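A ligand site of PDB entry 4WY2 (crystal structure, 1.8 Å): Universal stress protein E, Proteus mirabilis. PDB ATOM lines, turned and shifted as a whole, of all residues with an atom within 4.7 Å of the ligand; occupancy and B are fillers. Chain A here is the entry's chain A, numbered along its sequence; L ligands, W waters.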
ATOM      1  N   ASP A  19      -7.703   3.459 -16.098  1.00  0.00           N
ATOM      2  CA  ASP A  19      -8.861   2.614 -16.353  1.00  0.00           C
ATOM      3  C   ASP A  19      -8.512   1.380 -17.128  1.00  0.00           C
ATOM      4  O   ASP A  19      -8.770   0.276 -16.672  1.00  0.00           O
ATOM      5  CB  ASP A  19      -9.955   3.384 -17.089  1.00  0.00           C
ATOM      6  CG  ASP A  19     -10.593   4.464 -16.213  1.00  0.00           C
ATOM      7  OD1 ASP A  19     -10.586   4.344 -14.985  1.00  0.00           O
ATOM      8  OD2 ASP A  19     -11.106   5.434 -16.786  1.00  0.00           O
ATOM      9  N   ASP A  20      -7.941   1.566 -18.322  1.00  0.00           N
ATOM     10  CA  ASP A  20      -7.655   0.435 -19.189  1.00  0.00           C
ATOM     11  C   ASP A  20      -6.631  -0.499 -18.525  1.00  0.00           C
ATOM     12  O   ASP A  20      -5.676  -0.031 -17.926  1.00  0.00           O
ATOM     13  CB  ASP A  20      -7.101   0.889 -20.549  1.00  0.00           C
ATOM     14  CG  ASP A  20      -6.939  -0.249 -21.509  1.00  0.00           C
ATOM     15  OD1 ASP A  20      -7.962  -0.877 -21.847  1.00  0.00           O
ATOM     16  OD2 ASP A  20      -5.805  -0.567 -21.912  1.00  0.00           O
ATOM     17  N   GLN A  21      -6.837  -1.808 -18.672  1.00  0.00           N
ATOM     18  CA  GLN A  21      -6.054  -2.830 -18.005  1.00  0.00           C
ATOM     19  C   GLN A  21      -5.411  -3.764 -19.014  1.00  0.00           C
ATOM     20  O   GLN A  21      -5.965  -4.822 -19.384  1.00  0.00           O
ATOM     21  CB  GLN A  21      -6.944  -3.600 -17.017  1.00  0.00           C
ATOM     22  CG  GLN A  21      -7.562  -2.732 -15.944  1.00  0.00           C
ATOM     23  CD  GLN A  21      -6.524  -2.124 -15.005  1.00  0.00           C
ATOM     24  OE1 GLN A  21      -5.580  -2.798 -14.644  1.00  0.00           O
ATOM     25  NE2 GLN A  21      -6.685  -0.861 -14.643  1.00  0.00           N
ATOM     26  N   LEU A  24      -5.329  -7.375 -17.880  1.00  0.00           N
ATOM     27  CA  LEU A  24      -6.612  -8.081 -18.074  1.00  0.00           C
ATOM     28  C   LEU A  24      -6.841  -8.508 -19.501  1.00  0.00           C
ATOM     29  O   LEU A  24      -7.276  -9.634 -19.777  1.00  0.00           O
ATOM     30  CB  LEU A  24      -7.799  -7.229 -17.662  1.00  0.00           C
ATOM     31  CG  LEU A  24      -9.160  -7.928 -17.606  1.00  0.00           C
ATOM     32  CD1 LEU A  24      -9.175  -9.153 -16.727  1.00  0.00           C
ATOM     33  CD2 LEU A  24     -10.215  -6.949 -17.112  1.00  0.00           C
ATOM     34  N   ARG A  25      -6.574  -7.603 -20.438  1.00  0.00           N
ATOM     35  CA  ARG A  25      -6.682  -7.913 -21.859  1.00  0.00           C
ATOM     36  C   ARG A  25      -5.852  -9.140 -22.255  1.00  0.00           C
ATOM     37  O   ARG A  25      -6.335 -10.066 -22.967  1.00  0.00           O
ATOM     38  CB  ARG A  25      -6.288  -6.696 -22.678  1.00  0.00           C
ATOM     39  CG  ARG A  25      -6.329  -6.901 -24.174  1.00  0.00           C
ATOM     40  CD  ARG A  25      -5.992  -5.631 -24.932  1.00  0.00           C
ATOM     41  NE  ARG A  25      -7.050  -4.648 -24.783  1.00  0.00           N
ATOM     42  CZ  ARG A  25      -7.023  -3.571 -23.993  1.00  0.00           C
ATOM     43  NH1 ARG A  25      -8.085  -2.776 -23.950  1.00  0.00           N
ATOM     44  NH2 ARG A  25      -5.967  -3.276 -23.242  1.00  0.00           N
ATOM     45  N   ARG A  26      -4.593  -9.192 -21.782  1.00  0.00           N
ATOM     46  CA  ARG A  26      -3.715 -10.282 -22.106  1.00  0.00           C
ATOM     47  C   ARG A  26      -4.275 -11.579 -21.556  1.00  0.00           C
ATOM     48  O   ARG A  26      -4.250 -12.617 -22.246  1.00  0.00           O
ATOM     49  CB  ARG A  26      -2.284 -10.069 -21.599  1.00  0.00           C
ATOM     50  CG  ARG A  26      -1.350 -11.252 -21.882  1.00  0.00           C
ATOM     51  CD  ARG A  26      -1.139 -11.520 -23.375  1.00  0.00           C
ATOM     52  NE  ARG A  26      -0.930 -10.282 -24.122  1.00  0.00           N
ATOM     53  CZ  ARG A  26       0.220  -9.618 -24.201  1.00  0.00           C
ATOM     54  NH1 ARG A  26       0.273  -8.465 -24.857  1.00  0.00           N
ATOM     55  NH2 ARG A  26       1.324 -10.057 -23.608  1.00  0.00           N
ATOM     56  N   VAL A  28      -7.373 -12.318 -20.977  1.00  0.00           N
ATOM     57  CA  VAL A  28      -8.541 -12.680 -21.777  1.00  0.00           C
ATOM     58  C   VAL A  28      -8.103 -13.359 -23.067  1.00  0.00           C
ATOM     59  O   VAL A  28      -8.677 -14.402 -23.485  1.00  0.00           O
ATOM     60  CB  VAL A  28      -9.433 -11.471 -22.091  1.00  0.00           C
ATOM     61  CG1 VAL A  28     -10.456 -11.789 -23.192  1.00  0.00           C
ATOM     62  CG2 VAL A  28     -10.138 -11.037 -20.835  1.00  0.00           C
ATOM     63  N   TYR A  29      -7.109 -12.779 -23.717  1.00  0.00           N
ATOM     64  CA  TYR A  29      -6.580 -13.354 -24.937  1.00  0.00           C
ATOM     65  C   TYR A  29      -6.170 -14.822 -24.692  1.00  0.00           C
ATOM     66  O   TYR A  29      -6.427 -15.723 -25.537  1.00  0.00           O
ATOM     67  CB  TYR A  29      -5.376 -12.522 -25.400  1.00  0.00           C
ATOM     68  CG  TYR A  29      -4.778 -13.001 -26.683  1.00  0.00           C
ATOM     69  CD1 TYR A  29      -5.273 -12.535 -27.891  1.00  0.00           C
ATOM     70  CD2 TYR A  29      -3.761 -13.935 -26.696  1.00  0.00           C
ATOM     71  CE1 TYR A  29      -4.743 -12.965 -29.097  1.00  0.00           C
ATOM     72  CE2 TYR A  29      -3.241 -14.397 -27.905  1.00  0.00           C
ATOM     73  CZ  TYR A  29      -3.726 -13.880 -29.079  1.00  0.00           C
ATOM     74  OH  TYR A  29      -3.215 -14.309 -30.272  1.00  0.00           O
ATOM     75  N   GLN A  32      -9.357 -17.204 -23.988  1.00  0.00           N
ATOM     76  CA  GLN A  32     -10.111 -17.437 -25.212  1.00  0.00           C
ATOM     77  C   GLN A  32      -9.495 -18.566 -26.016  1.00  0.00           C
ATOM     78  O   GLN A  32     -10.196 -19.272 -26.762  1.00  0.00           O
ATOM     79  CB  GLN A  32     -10.083 -16.216 -26.095  1.00  0.00           C
ATOM     80  CG  GLN A  32     -10.904 -15.045 -25.618  1.00  0.00           C
ATOM     81  CD  GLN A  32     -10.668 -13.808 -26.447  1.00  0.00           C
ATOM     82  OE1 GLN A  32      -9.625 -13.656 -27.090  1.00  0.00           O
ATOM     83  NE2 GLN A  32     -11.639 -12.891 -26.443  1.00  0.00           N
ATOM     84  N   GLN A  77     -16.743  -2.469 -14.448  1.00  0.00           N
ATOM     85  CA  GLN A  77     -16.918  -1.572 -15.593  1.00  0.00           C
ATOM     86  C   GLN A  77     -15.857  -1.812 -16.663  1.00  0.00           C
ATOM     87  O   GLN A  77     -16.168  -1.971 -17.822  1.00  0.00           O
ATOM     88  CB  GLN A  77     -16.912  -0.101 -15.141  1.00  0.00           C
ATOM     89  CG  GLN A  77     -17.341   0.862 -16.252  1.00  0.00           C
ATOM     90  N   GLN A  78     -14.596  -1.937 -16.260  1.00  0.00           N
ATOM     91  CA  GLN A  78     -13.523  -2.274 -17.208  1.00  0.00           C
ATOM     92  C   GLN A  78     -13.682  -3.672 -17.815  1.00  0.00           C
ATOM     93  O   GLN A  78     -13.388  -3.869 -19.000  1.00  0.00           O
ATOM     94  CB  GLN A  78     -12.160  -2.153 -16.523  1.00  0.00           C
ATOM     95  CG  GLN A  78     -11.859  -0.800 -15.914  1.00  0.00           C
ATOM     96  CD  GLN A  78     -12.150   0.349 -16.859  1.00  0.00           C
ATOM     97  OE1 GLN A  78     -11.688   0.385 -17.996  1.00  0.00           O
ATOM     98  NE2 GLN A  78     -12.951   1.289 -16.381  1.00  0.00           N
ATOM     99  N   TYR A  81     -17.267  -5.894 -21.112  1.00  0.00           N
ATOM    100  CA  TYR A  81     -17.378  -6.528 -22.448  1.00  0.00           C
ATOM    101  C   TYR A  81     -16.874  -7.979 -22.421  1.00  0.00           C
ATOM    102  O   TYR A  81     -17.478  -8.885 -23.051  1.00  0.00           O
ATOM    103  CB  TYR A  81     -16.652  -5.702 -23.516  1.00  0.00           C
ATOM    104  CG  TYR A  81     -17.339  -4.372 -23.735  1.00  0.00           C
ATOM    105  CD1 TYR A  81     -18.480  -4.277 -24.566  1.00  0.00           C
ATOM    106  CD2 TYR A  81     -16.884  -3.216 -23.119  1.00  0.00           C
ATOM    107  CE1 TYR A  81     -19.126  -3.070 -24.764  1.00  0.00           C
ATOM    108  CE2 TYR A  81     -17.520  -1.999 -23.320  1.00  0.00           C
ATOM    109  CZ  TYR A  81     -18.645  -1.925 -24.133  1.00  0.00           C
ATOM    110  OH  TYR A  81     -19.287  -0.710 -24.326  1.00  0.00           O
ATOM    111  N   TYR A  82     -15.789  -8.215 -21.709  1.00  0.00           N
ATOM    112  CA  TYR A  82     -15.272  -9.578 -21.508  1.00  0.00           C
ATOM    113  C   TYR A  82     -16.289 -10.482 -20.815  1.00  0.00           C
ATOM    114  O   TYR A  82     -16.537 -11.618 -21.261  1.00  0.00           O
ATOM    115  CB  TYR A  82     -13.956  -9.555 -20.695  1.00  0.00           C
ATOM    116  CG  TYR A  82     -12.831  -8.741 -21.309  1.00  0.00           C
ATOM    117  CD1 TYR A  82     -12.542  -8.813 -22.666  1.00  0.00           C
ATOM    118  CD2 TYR A  82     -12.054  -7.891 -20.506  1.00  0.00           C
ATOM    119  CE1 TYR A  82     -11.512  -8.059 -23.215  1.00  0.00           C
ATOM    120  CE2 TYR A  82     -11.036  -7.141 -21.038  1.00  0.00           C
ATOM    121  CZ  TYR A  82     -10.758  -7.218 -22.380  1.00  0.00           C
ATOM    122  OH  TYR A  82      -9.738  -6.479 -22.876  1.00  0.00           O
ATOM    123  N   TRP A 146       4.406 -12.524 -15.513  1.00  0.00           N
ATOM    124  CA  TRP A 146       4.347 -12.014 -16.886  1.00  0.00           C
ATOM    125  C   TRP A 146       4.122 -10.501 -16.844  1.00  0.00           C
ATOM    126  O   TRP A 146       3.019 -10.031 -16.503  1.00  0.00           O
ATOM    127  CB  TRP A 146       3.208 -12.681 -17.636  1.00  0.00           C
ATOM    128  CG  TRP A 146       3.155 -12.462 -19.162  1.00  0.00           C
ATOM    129  CD1 TRP A 146       3.631 -11.382 -19.871  1.00  0.00           C
ATOM    130  CD2 TRP A 146       2.536 -13.323 -20.132  1.00  0.00           C
ATOM    131  NE1 TRP A 146       3.377 -11.546 -21.206  1.00  0.00           N
ATOM    132  CE2 TRP A 146       2.681 -12.716 -21.392  1.00  0.00           C
ATOM    133  CE3 TRP A 146       1.892 -14.556 -20.057  1.00  0.00           C
ATOM    134  CZ2 TRP A 146       2.238 -13.307 -22.578  1.00  0.00           C
ATOM    135  CZ3 TRP A 146       1.434 -15.138 -21.226  1.00  0.00           C
ATOM    136  CH2 TRP A 146       1.605 -14.520 -22.464  1.00  0.00           C
ATOM    137  N   TRP A 153       1.349  -5.930 -29.227  1.00  0.00           N
ATOM    138  CA  TRP A 153       2.220  -7.052 -29.475  1.00  0.00           C
ATOM    139  C   TRP A 153       2.680  -6.956 -30.927  1.00  0.00           C
ATOM    140  O   TRP A 153       1.863  -6.739 -31.818  1.00  0.00           O
ATOM    141  CB  TRP A 153       1.464  -8.344 -29.245  1.00  0.00           C
ATOM    142  CG  TRP A 153       2.263  -9.578 -29.424  1.00  0.00           C
ATOM    143  CD1 TRP A 153       2.420 -10.296 -30.575  1.00  0.00           C
ATOM    144  CD2 TRP A 153       2.974 -10.287 -28.406  1.00  0.00           C
ATOM    145  NE1 TRP A 153       3.201 -11.400 -30.339  1.00  0.00           N
ATOM    146  CE2 TRP A 153       3.573 -11.403 -29.016  1.00  0.00           C
ATOM    147  CE3 TRP A 153       3.191 -10.069 -27.045  1.00  0.00           C
ATOM    148  CZ2 TRP A 153       4.335 -12.316 -28.321  1.00  0.00           C
ATOM    149  CZ3 TRP A 153       3.949 -10.968 -26.349  1.00  0.00           C
ATOM    150  CH2 TRP A 153       4.509 -12.092 -26.977  1.00  0.00           C
ATOM    151  N   ILE A 159       9.331 -15.389 -29.644  1.00  0.00           N
ATOM    152  CA  ILE A 159       9.387 -15.742 -28.230  1.00  0.00           C
ATOM    153  C   ILE A 159      10.841 -16.129 -27.949  1.00  0.00           C
ATOM    154  O   ILE A 159      11.330 -17.119 -28.491  1.00  0.00           O
ATOM    155  CB  ILE A 159       8.408 -16.912 -27.937  1.00  0.00           C
ATOM    156  CG1 ILE A 159       6.977 -16.492 -28.268  1.00  0.00           C
ATOM    157  CG2 ILE A 159       8.456 -17.316 -26.480  1.00  0.00           C
ATOM    158  CD1 ILE A 159       6.018 -17.652 -28.466  1.00  0.00           C
ATOM    159  N   THR A 183       7.788 -22.664 -22.013  1.00  0.00           N
ATOM    160  CA  THR A 183       7.628 -21.797 -23.182  1.00  0.00           C
ATOM    161  C   THR A 183       6.984 -22.574 -24.324  1.00  0.00           C
ATOM    162  O   THR A 183       6.055 -22.108 -24.974  1.00  0.00           O
ATOM    163  CB  THR A 183       8.975 -21.217 -23.624  1.00  0.00           C
ATOM    164  OG1 THR A 183       9.461 -20.338 -22.580  1.00  0.00           O
ATOM    165  CG2 THR A 183       8.846 -20.453 -24.939  1.00  0.00           C
ATOM    166  N   LEU A 186       3.089 -23.506 -23.188  1.00  0.00           N
ATOM    167  CA  LEU A 186       2.206 -22.344 -23.153  1.00  0.00           C
ATOM    168  C   LEU A 186       2.068 -21.656 -24.521  1.00  0.00           C
ATOM    169  O   LEU A 186       0.975 -21.274 -24.894  1.00  0.00           O
ATOM    170  CB  LEU A 186       2.717 -21.319 -22.114  1.00  0.00           C
ATOM    171  CG  LEU A 186       1.898 -20.048 -21.837  1.00  0.00           C
ATOM    172  CD1 LEU A 186       0.444 -20.334 -21.530  1.00  0.00           C
ATOM    173  CD2 LEU A 186       2.523 -19.238 -20.712  1.00  0.00           C
ATOM    174  N   SER A 187       3.167 -21.496 -25.261  1.00  0.00           N
ATOM    175  CA  SER A 187       3.095 -20.800 -26.553  1.00  0.00           C
ATOM    176  C   SER A 187       2.195 -21.553 -27.533  1.00  0.00           C
ATOM    177  O   SER A 187       1.488 -20.945 -28.336  1.00  0.00           O
ATOM    178  CB  SER A 187       4.469 -20.569 -27.174  1.00  0.00           C
ATOM    179  OG  SER A 187       5.173 -21.753 -27.498  1.00  0.00           O
ATOM    180  N   ILE A 190      -1.495 -21.016 -26.980  1.00  0.00           N
ATOM    181  CA  ILE A 190      -1.947 -19.667 -27.250  1.00  0.00           C
ATOM    182  C   ILE A 190      -1.846 -19.285 -28.707  1.00  0.00           C
ATOM    183  O   ILE A 190      -2.739 -18.627 -29.225  1.00  0.00           O
ATOM    184  CB  ILE A 190      -1.121 -18.654 -26.416  1.00  0.00           C
ATOM    185  CG1 ILE A 190      -1.337 -18.954 -24.957  1.00  0.00           C
ATOM    186  CG2 ILE A 190      -1.510 -17.226 -26.797  1.00  0.00           C
ATOM    187  CD1 ILE A 190      -0.582 -17.981 -24.047  1.00  0.00           C
ATOM    188  N   GLN A 191      -0.792 -19.740 -29.397  1.00  0.00           N
ATOM    189  CA  GLN A 191      -0.536 -19.351 -30.764  1.00  0.00           C
ATOM    190  C   GLN A 191      -0.590 -20.593 -31.657  1.00  0.00           C
ATOM    191  O   GLN A 191      -0.180 -21.673 -31.253  1.00  0.00           O
ATOM    192  CB  GLN A 191       0.850 -18.719 -30.896  1.00  0.00           C
ATOM    193  CG  GLN A 191       1.014 -17.451 -30.068  1.00  0.00           C
ATOM    194  CD  GLN A 191       2.206 -16.643 -30.546  1.00  0.00           C
ATOM    195  OE1 GLN A 191       3.328 -17.126 -30.561  1.00  0.00           O
ATOM    196  NE2 GLN A 191       1.966 -15.382 -30.942  1.00  0.00           N
ATOM    197  N   ILE A 269       8.347 -11.195 -26.427  1.00  0.00           N
ATOM    198  CA  ILE A 269       8.550 -11.539 -25.043  1.00  0.00           C
ATOM    199  C   ILE A 269       9.908 -12.195 -24.870  1.00  0.00           C
ATOM    200  O   ILE A 269      10.421 -12.877 -25.789  1.00  0.00           O
ATOM    201  CB  ILE A 269       7.394 -12.450 -24.554  1.00  0.00           C
ATOM    202  CG1 ILE A 269       7.448 -12.644 -23.046  1.00  0.00           C
ATOM    203  CG2 ILE A 269       7.376 -13.768 -25.315  1.00  0.00           C
ATOM    204  CD1 ILE A 269       6.129 -13.143 -22.472  1.00  0.00           C
ATOM    205  N   LEU A 301       8.633 -12.673 -19.158  1.00  0.00           N
ATOM    206  CA  LEU A 301       8.107 -13.778 -18.390  1.00  0.00           C
ATOM    207  C   LEU A 301       9.229 -14.321 -17.508  1.00  0.00           C
ATOM    208  O   LEU A 301      10.184 -14.936 -18.010  1.00  0.00           O
ATOM    209  CB  LEU A 301       7.527 -14.853 -19.316  1.00  0.00           C
ATOM    210  CG  LEU A 301       6.887 -16.028 -18.575  1.00  0.00           C
ATOM    211  CD1 LEU A 301       5.649 -15.644 -17.773  1.00  0.00           C
ATOM    212  CD2 LEU A 301       6.513 -17.101 -19.604  1.00  0.00           C
HETATM  213  C1  LIG L   1      -5.769  -6.035 -30.261  1.00  0.00           C
HETATM  214  C2  LIG L   1      -6.692  -4.817 -30.303  1.00  0.00           C
HETATM  215  C3  LIG L   1      -6.340  -3.796 -31.385  1.00  0.00           C
HETATM  216  N1  LIG L   1      -8.011  -7.892 -27.795  1.00  0.00           N
HETATM  217  C4  LIG L   1      -6.169  -6.923 -29.087  1.00  0.00           C
HETATM  218  C5  LIG L   1       5.544 -18.480 -23.511  1.00  0.00           C
HETATM  219  C6  LIG L   1       4.719 -17.218 -23.457  1.00  0.00           C
HETATM  220  C7  LIG L   1       4.490 -16.639 -24.846  1.00  0.00           C
HETATM  221  C8  LIG L   1       3.146 -17.051 -25.433  1.00  0.00           C
HETATM  222  C9  LIG L   1       2.790 -16.158 -26.611  1.00  0.00           C
HETATM  223  C10 LIG L   1       1.880 -15.027 -26.186  1.00  0.00           C
HETATM  224  C11 LIG L   1       1.357 -14.274 -27.398  1.00  0.00           C
HETATM  225  C12 LIG L   1       0.426 -13.123 -27.007  1.00  0.00           C
HETATM  226  C13 LIG L   1      -0.015 -12.385 -28.240  1.00  0.00           C
HETATM  227  C14 LIG L   1      -0.959 -11.249 -27.876  1.00  0.00           C
HETATM  228  C15 LIG L   1      -1.512 -10.566 -29.116  1.00  0.00           C
HETATM  229  C16 LIG L   1      -2.295  -9.311 -28.741  1.00  0.00           C
HETATM  230  O1  LIG L   1      -2.501  -8.502 -29.884  1.00  0.00           O
HETATM  231  C17 LIG L   1      -3.642  -9.673 -28.137  1.00  0.00           C
HETATM  232  C18 LIG L   1      -4.499  -8.427 -28.073  1.00  0.00           C
HETATM  233  O2  LIG L   1      -4.423  -7.654 -27.129  1.00  0.00           O
HETATM  234  O3  LIG L   1      -5.415  -8.134 -29.167  1.00  0.00           O
HETATM  235  C19 LIG L   1      -7.643  -7.273 -29.067  1.00  0.00           C
HETATM  236  C20 LIG L   1      -8.040  -9.208 -27.587  1.00  0.00           C
HETATM  237  C21 LIG L   1      -8.501  -9.704 -26.234  1.00  0.00           C
HETATM  238  O4  LIG L   1      -7.702 -10.013 -28.440  1.00  0.00           O
HETATM  239  O5  LIG L   1      -4.399  -5.604 -30.106  1.00  0.00           O
HETATM  240  O6  LIG L   1      -6.399  -4.407 -32.677  1.00  0.00           O
HETATM  241  O7  LIG L   1      -8.018  -5.303 -30.466  1.00  0.00           O
HETATM  242  C22 LIG L   1      -8.483  -6.014 -29.317  1.00  0.00           C
HETATM  243  O8  LIG L   1      -8.391  -5.147 -28.170  1.00  0.00           O
HETATM  244  P1  LIG L   1      -9.586  -4.114 -27.752  1.00  0.00           P
HETATM  245  O9  LIG L   1      -9.934  -3.295 -28.982  1.00  0.00           O
HETATM  246  O10 LIG L   1      -9.145  -3.322 -26.537  1.00  0.00           O
HETATM  247  O11 LIG L   1     -10.754  -5.164 -27.438  1.00  0.00           O
HETATM  248  P2  LIG L   1     -10.863  -6.203 -26.233  1.00  0.00           P
HETATM  249  O12 LIG L   1      -9.508  -6.419 -25.559  1.00  0.00           O
HETATM  250  O13 LIG L   1     -11.621  -7.447 -26.638  1.00  0.00           O
HETATM  251  O14 LIG L   1     -11.776  -5.337 -25.211  1.00  0.00           O
HETATM  252  C23 LIG L   1     -13.209  -5.451 -25.248  1.00  0.00           C
HETATM  253  C24 LIG L   1     -13.778  -4.103 -24.844  1.00  0.00           C
HETATM  254  O15 LIG L   1     -13.608  -3.953 -23.421  1.00  0.00           O
HETATM  255  C25 LIG L   1     -13.070  -2.933 -25.511  1.00  0.00           C
HETATM  256  O16 LIG L   1     -14.003  -1.949 -25.942  1.00  0.00           O
HETATM  257  C26 LIG L   1     -12.207  -2.369 -24.407  1.00  0.00           C
HETATM  258  O17 LIG L   1     -11.951  -0.972 -24.516  1.00  0.00           O
HETATM  259  C27 LIG L   1     -13.017  -2.678 -23.156  1.00  0.00           C
HETATM  260  N2  LIG L   1     -12.076  -2.713 -22.022  1.00  0.00           N
HETATM  261  C28 LIG L   1     -11.101  -3.654 -21.992  1.00  0.00           C
HETATM  262  C29 LIG L   1     -10.170  -3.704 -20.946  1.00  0.00           C
HETATM  263  C30 LIG L   1     -10.280  -2.742 -19.933  1.00  0.00           C
HETATM  264  O18 LIG L   1      -9.483  -2.736 -18.971  1.00  0.00           O
HETATM  265  N3  LIG L   1     -11.245  -1.810 -19.997  1.00  0.00           N
HETATM  266  C31 LIG L   1     -12.149  -1.758 -20.985  1.00  0.00           C
HETATM  267  O19 LIG L   1     -13.037  -0.864 -20.990  1.00  0.00           O
HETATM  268  O   HOH W   1     -14.368  -5.375 -21.074  1.00  0.00           O
HETATM  269  O   HOH W   2      -8.748 -12.404 -28.981  1.00  0.00           O
HETATM  270  O   HOH W   3      -2.995  -8.506 -25.095  1.00  0.00           O
HETATM  271  O   HOH W   4      -6.529 -10.047 -31.083  1.00  0.00           O
HETATM  272  O   HOH W   5      -4.113  -3.727 -27.230  1.00  0.00           O
HETATM  273  O   HOH W   6     -11.205   1.817 -20.467  1.00  0.00           O
HETATM  274  O   HOH W   7      -1.643  -6.092 -28.967  1.00  0.00           O
HETATM  275  O   HOH W   8      -6.595  -1.979 -27.031  1.00  0.00           O
HETATM  276  O   HOH W   9     -10.420   0.189 -22.391  1.00  0.00           O
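Water W3 lies within hydrogen-bond range of an oxygen (O2) of the ligand (2.6 Å) and the guanidinium group of Arg 26 (2.9 Å).
Water W2 lies within hydrogen-bond range of the side-chain amide oxygen (OE1) of Gln 32 (2.4 Å) and an oxygen (O4) of the ligand (2.7 Å).
Water W7 bridges O1 of the ligand (2.7 Å) and N of Trp 153 (3.0 Å).
Water W1 lies within hydrogen-bond range of the backbone carbonyl oxygen (O) of Gln 78, an oxygen (O15) of the ligand, the backbone NH (N) of Tyr 81 and the backbone NH (N) of Tyr 82.
Water W9 lies within hydrogen-bond range of OD1 of Asp 20 and O17 of the ligand.
Water W6 bridges the side-chain amide oxygen (OE1) of Gln 78 and an oxygen (O19) of the ligand.
Residues that only touch the ligand: Tyr 29 (3.3 Å), Tyr 81 (3.4 Å), Asp 20 (3.5 Å), Trp 153 (3.7 Å), Gln 191 (3.8 Å), Trp 146 (3.8 Å), Asp 19 (3.9 Å), Arg 26 (3.9 Å), Ser 187 (3.9 Å) and Thr 183 (3.9 Å).
Hydrophobic or aromatic side chains that line the ligand: Tyr 29, Tyr 81, Tyr 82, Trp 146 and Trp 153.
Within 4 Å of the ligand: Asp 19, Asp 20, Gln 21, Arg 25, Arg 26, Tyr 29, Gln 78, Tyr 81, Tyr 82, Trp 146, Trp 153, Thr 183, Ser 187 and Gln 191.
Along chain A the residues within 4 Å of the ligand span positions 19 to 191.
An oxygen (O18) of the ligand lies within hydrogen-bond range of the backbone NH of Gln 21 (2.8 Å).
The side-chain hydroxyl (OH) of Tyr 82 sits at hydrogen-bond distance from an oxygen (O12) of the ligand, 2.7 Å away.
The guanidinium group of Arg 25 is in salt-bridge range of an oxygen (O10) of the ligand (2.8 Å).
O of Gln 78 lies within hydrogen-bond range of N3 of the ligand, 3.1 Å away.
The side-chain amide oxygen (OE1) of Gln 78 lies within hydrogen-bond range of a nitrogen (N3) of the ligand (3.0 Å).
OG of Ser 187 is in hydrogen-bond range of O of Thr 183 (2.7 Å).
NH1 of Arg 25 lies within salt-bridge range of OD1 of Asp 20 (2.8 Å).
The side-chain amide nitrogen (NE2) of Gln 21 sits at hydrogen-bond distance from the backbone carbonyl oxygen (O) of Asp 19.
The side-chain amide oxygen (OE1) of Gln 78 lies close to the backbone carbonyl oxygen (O) of Asp 19, at 3.2 Å.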
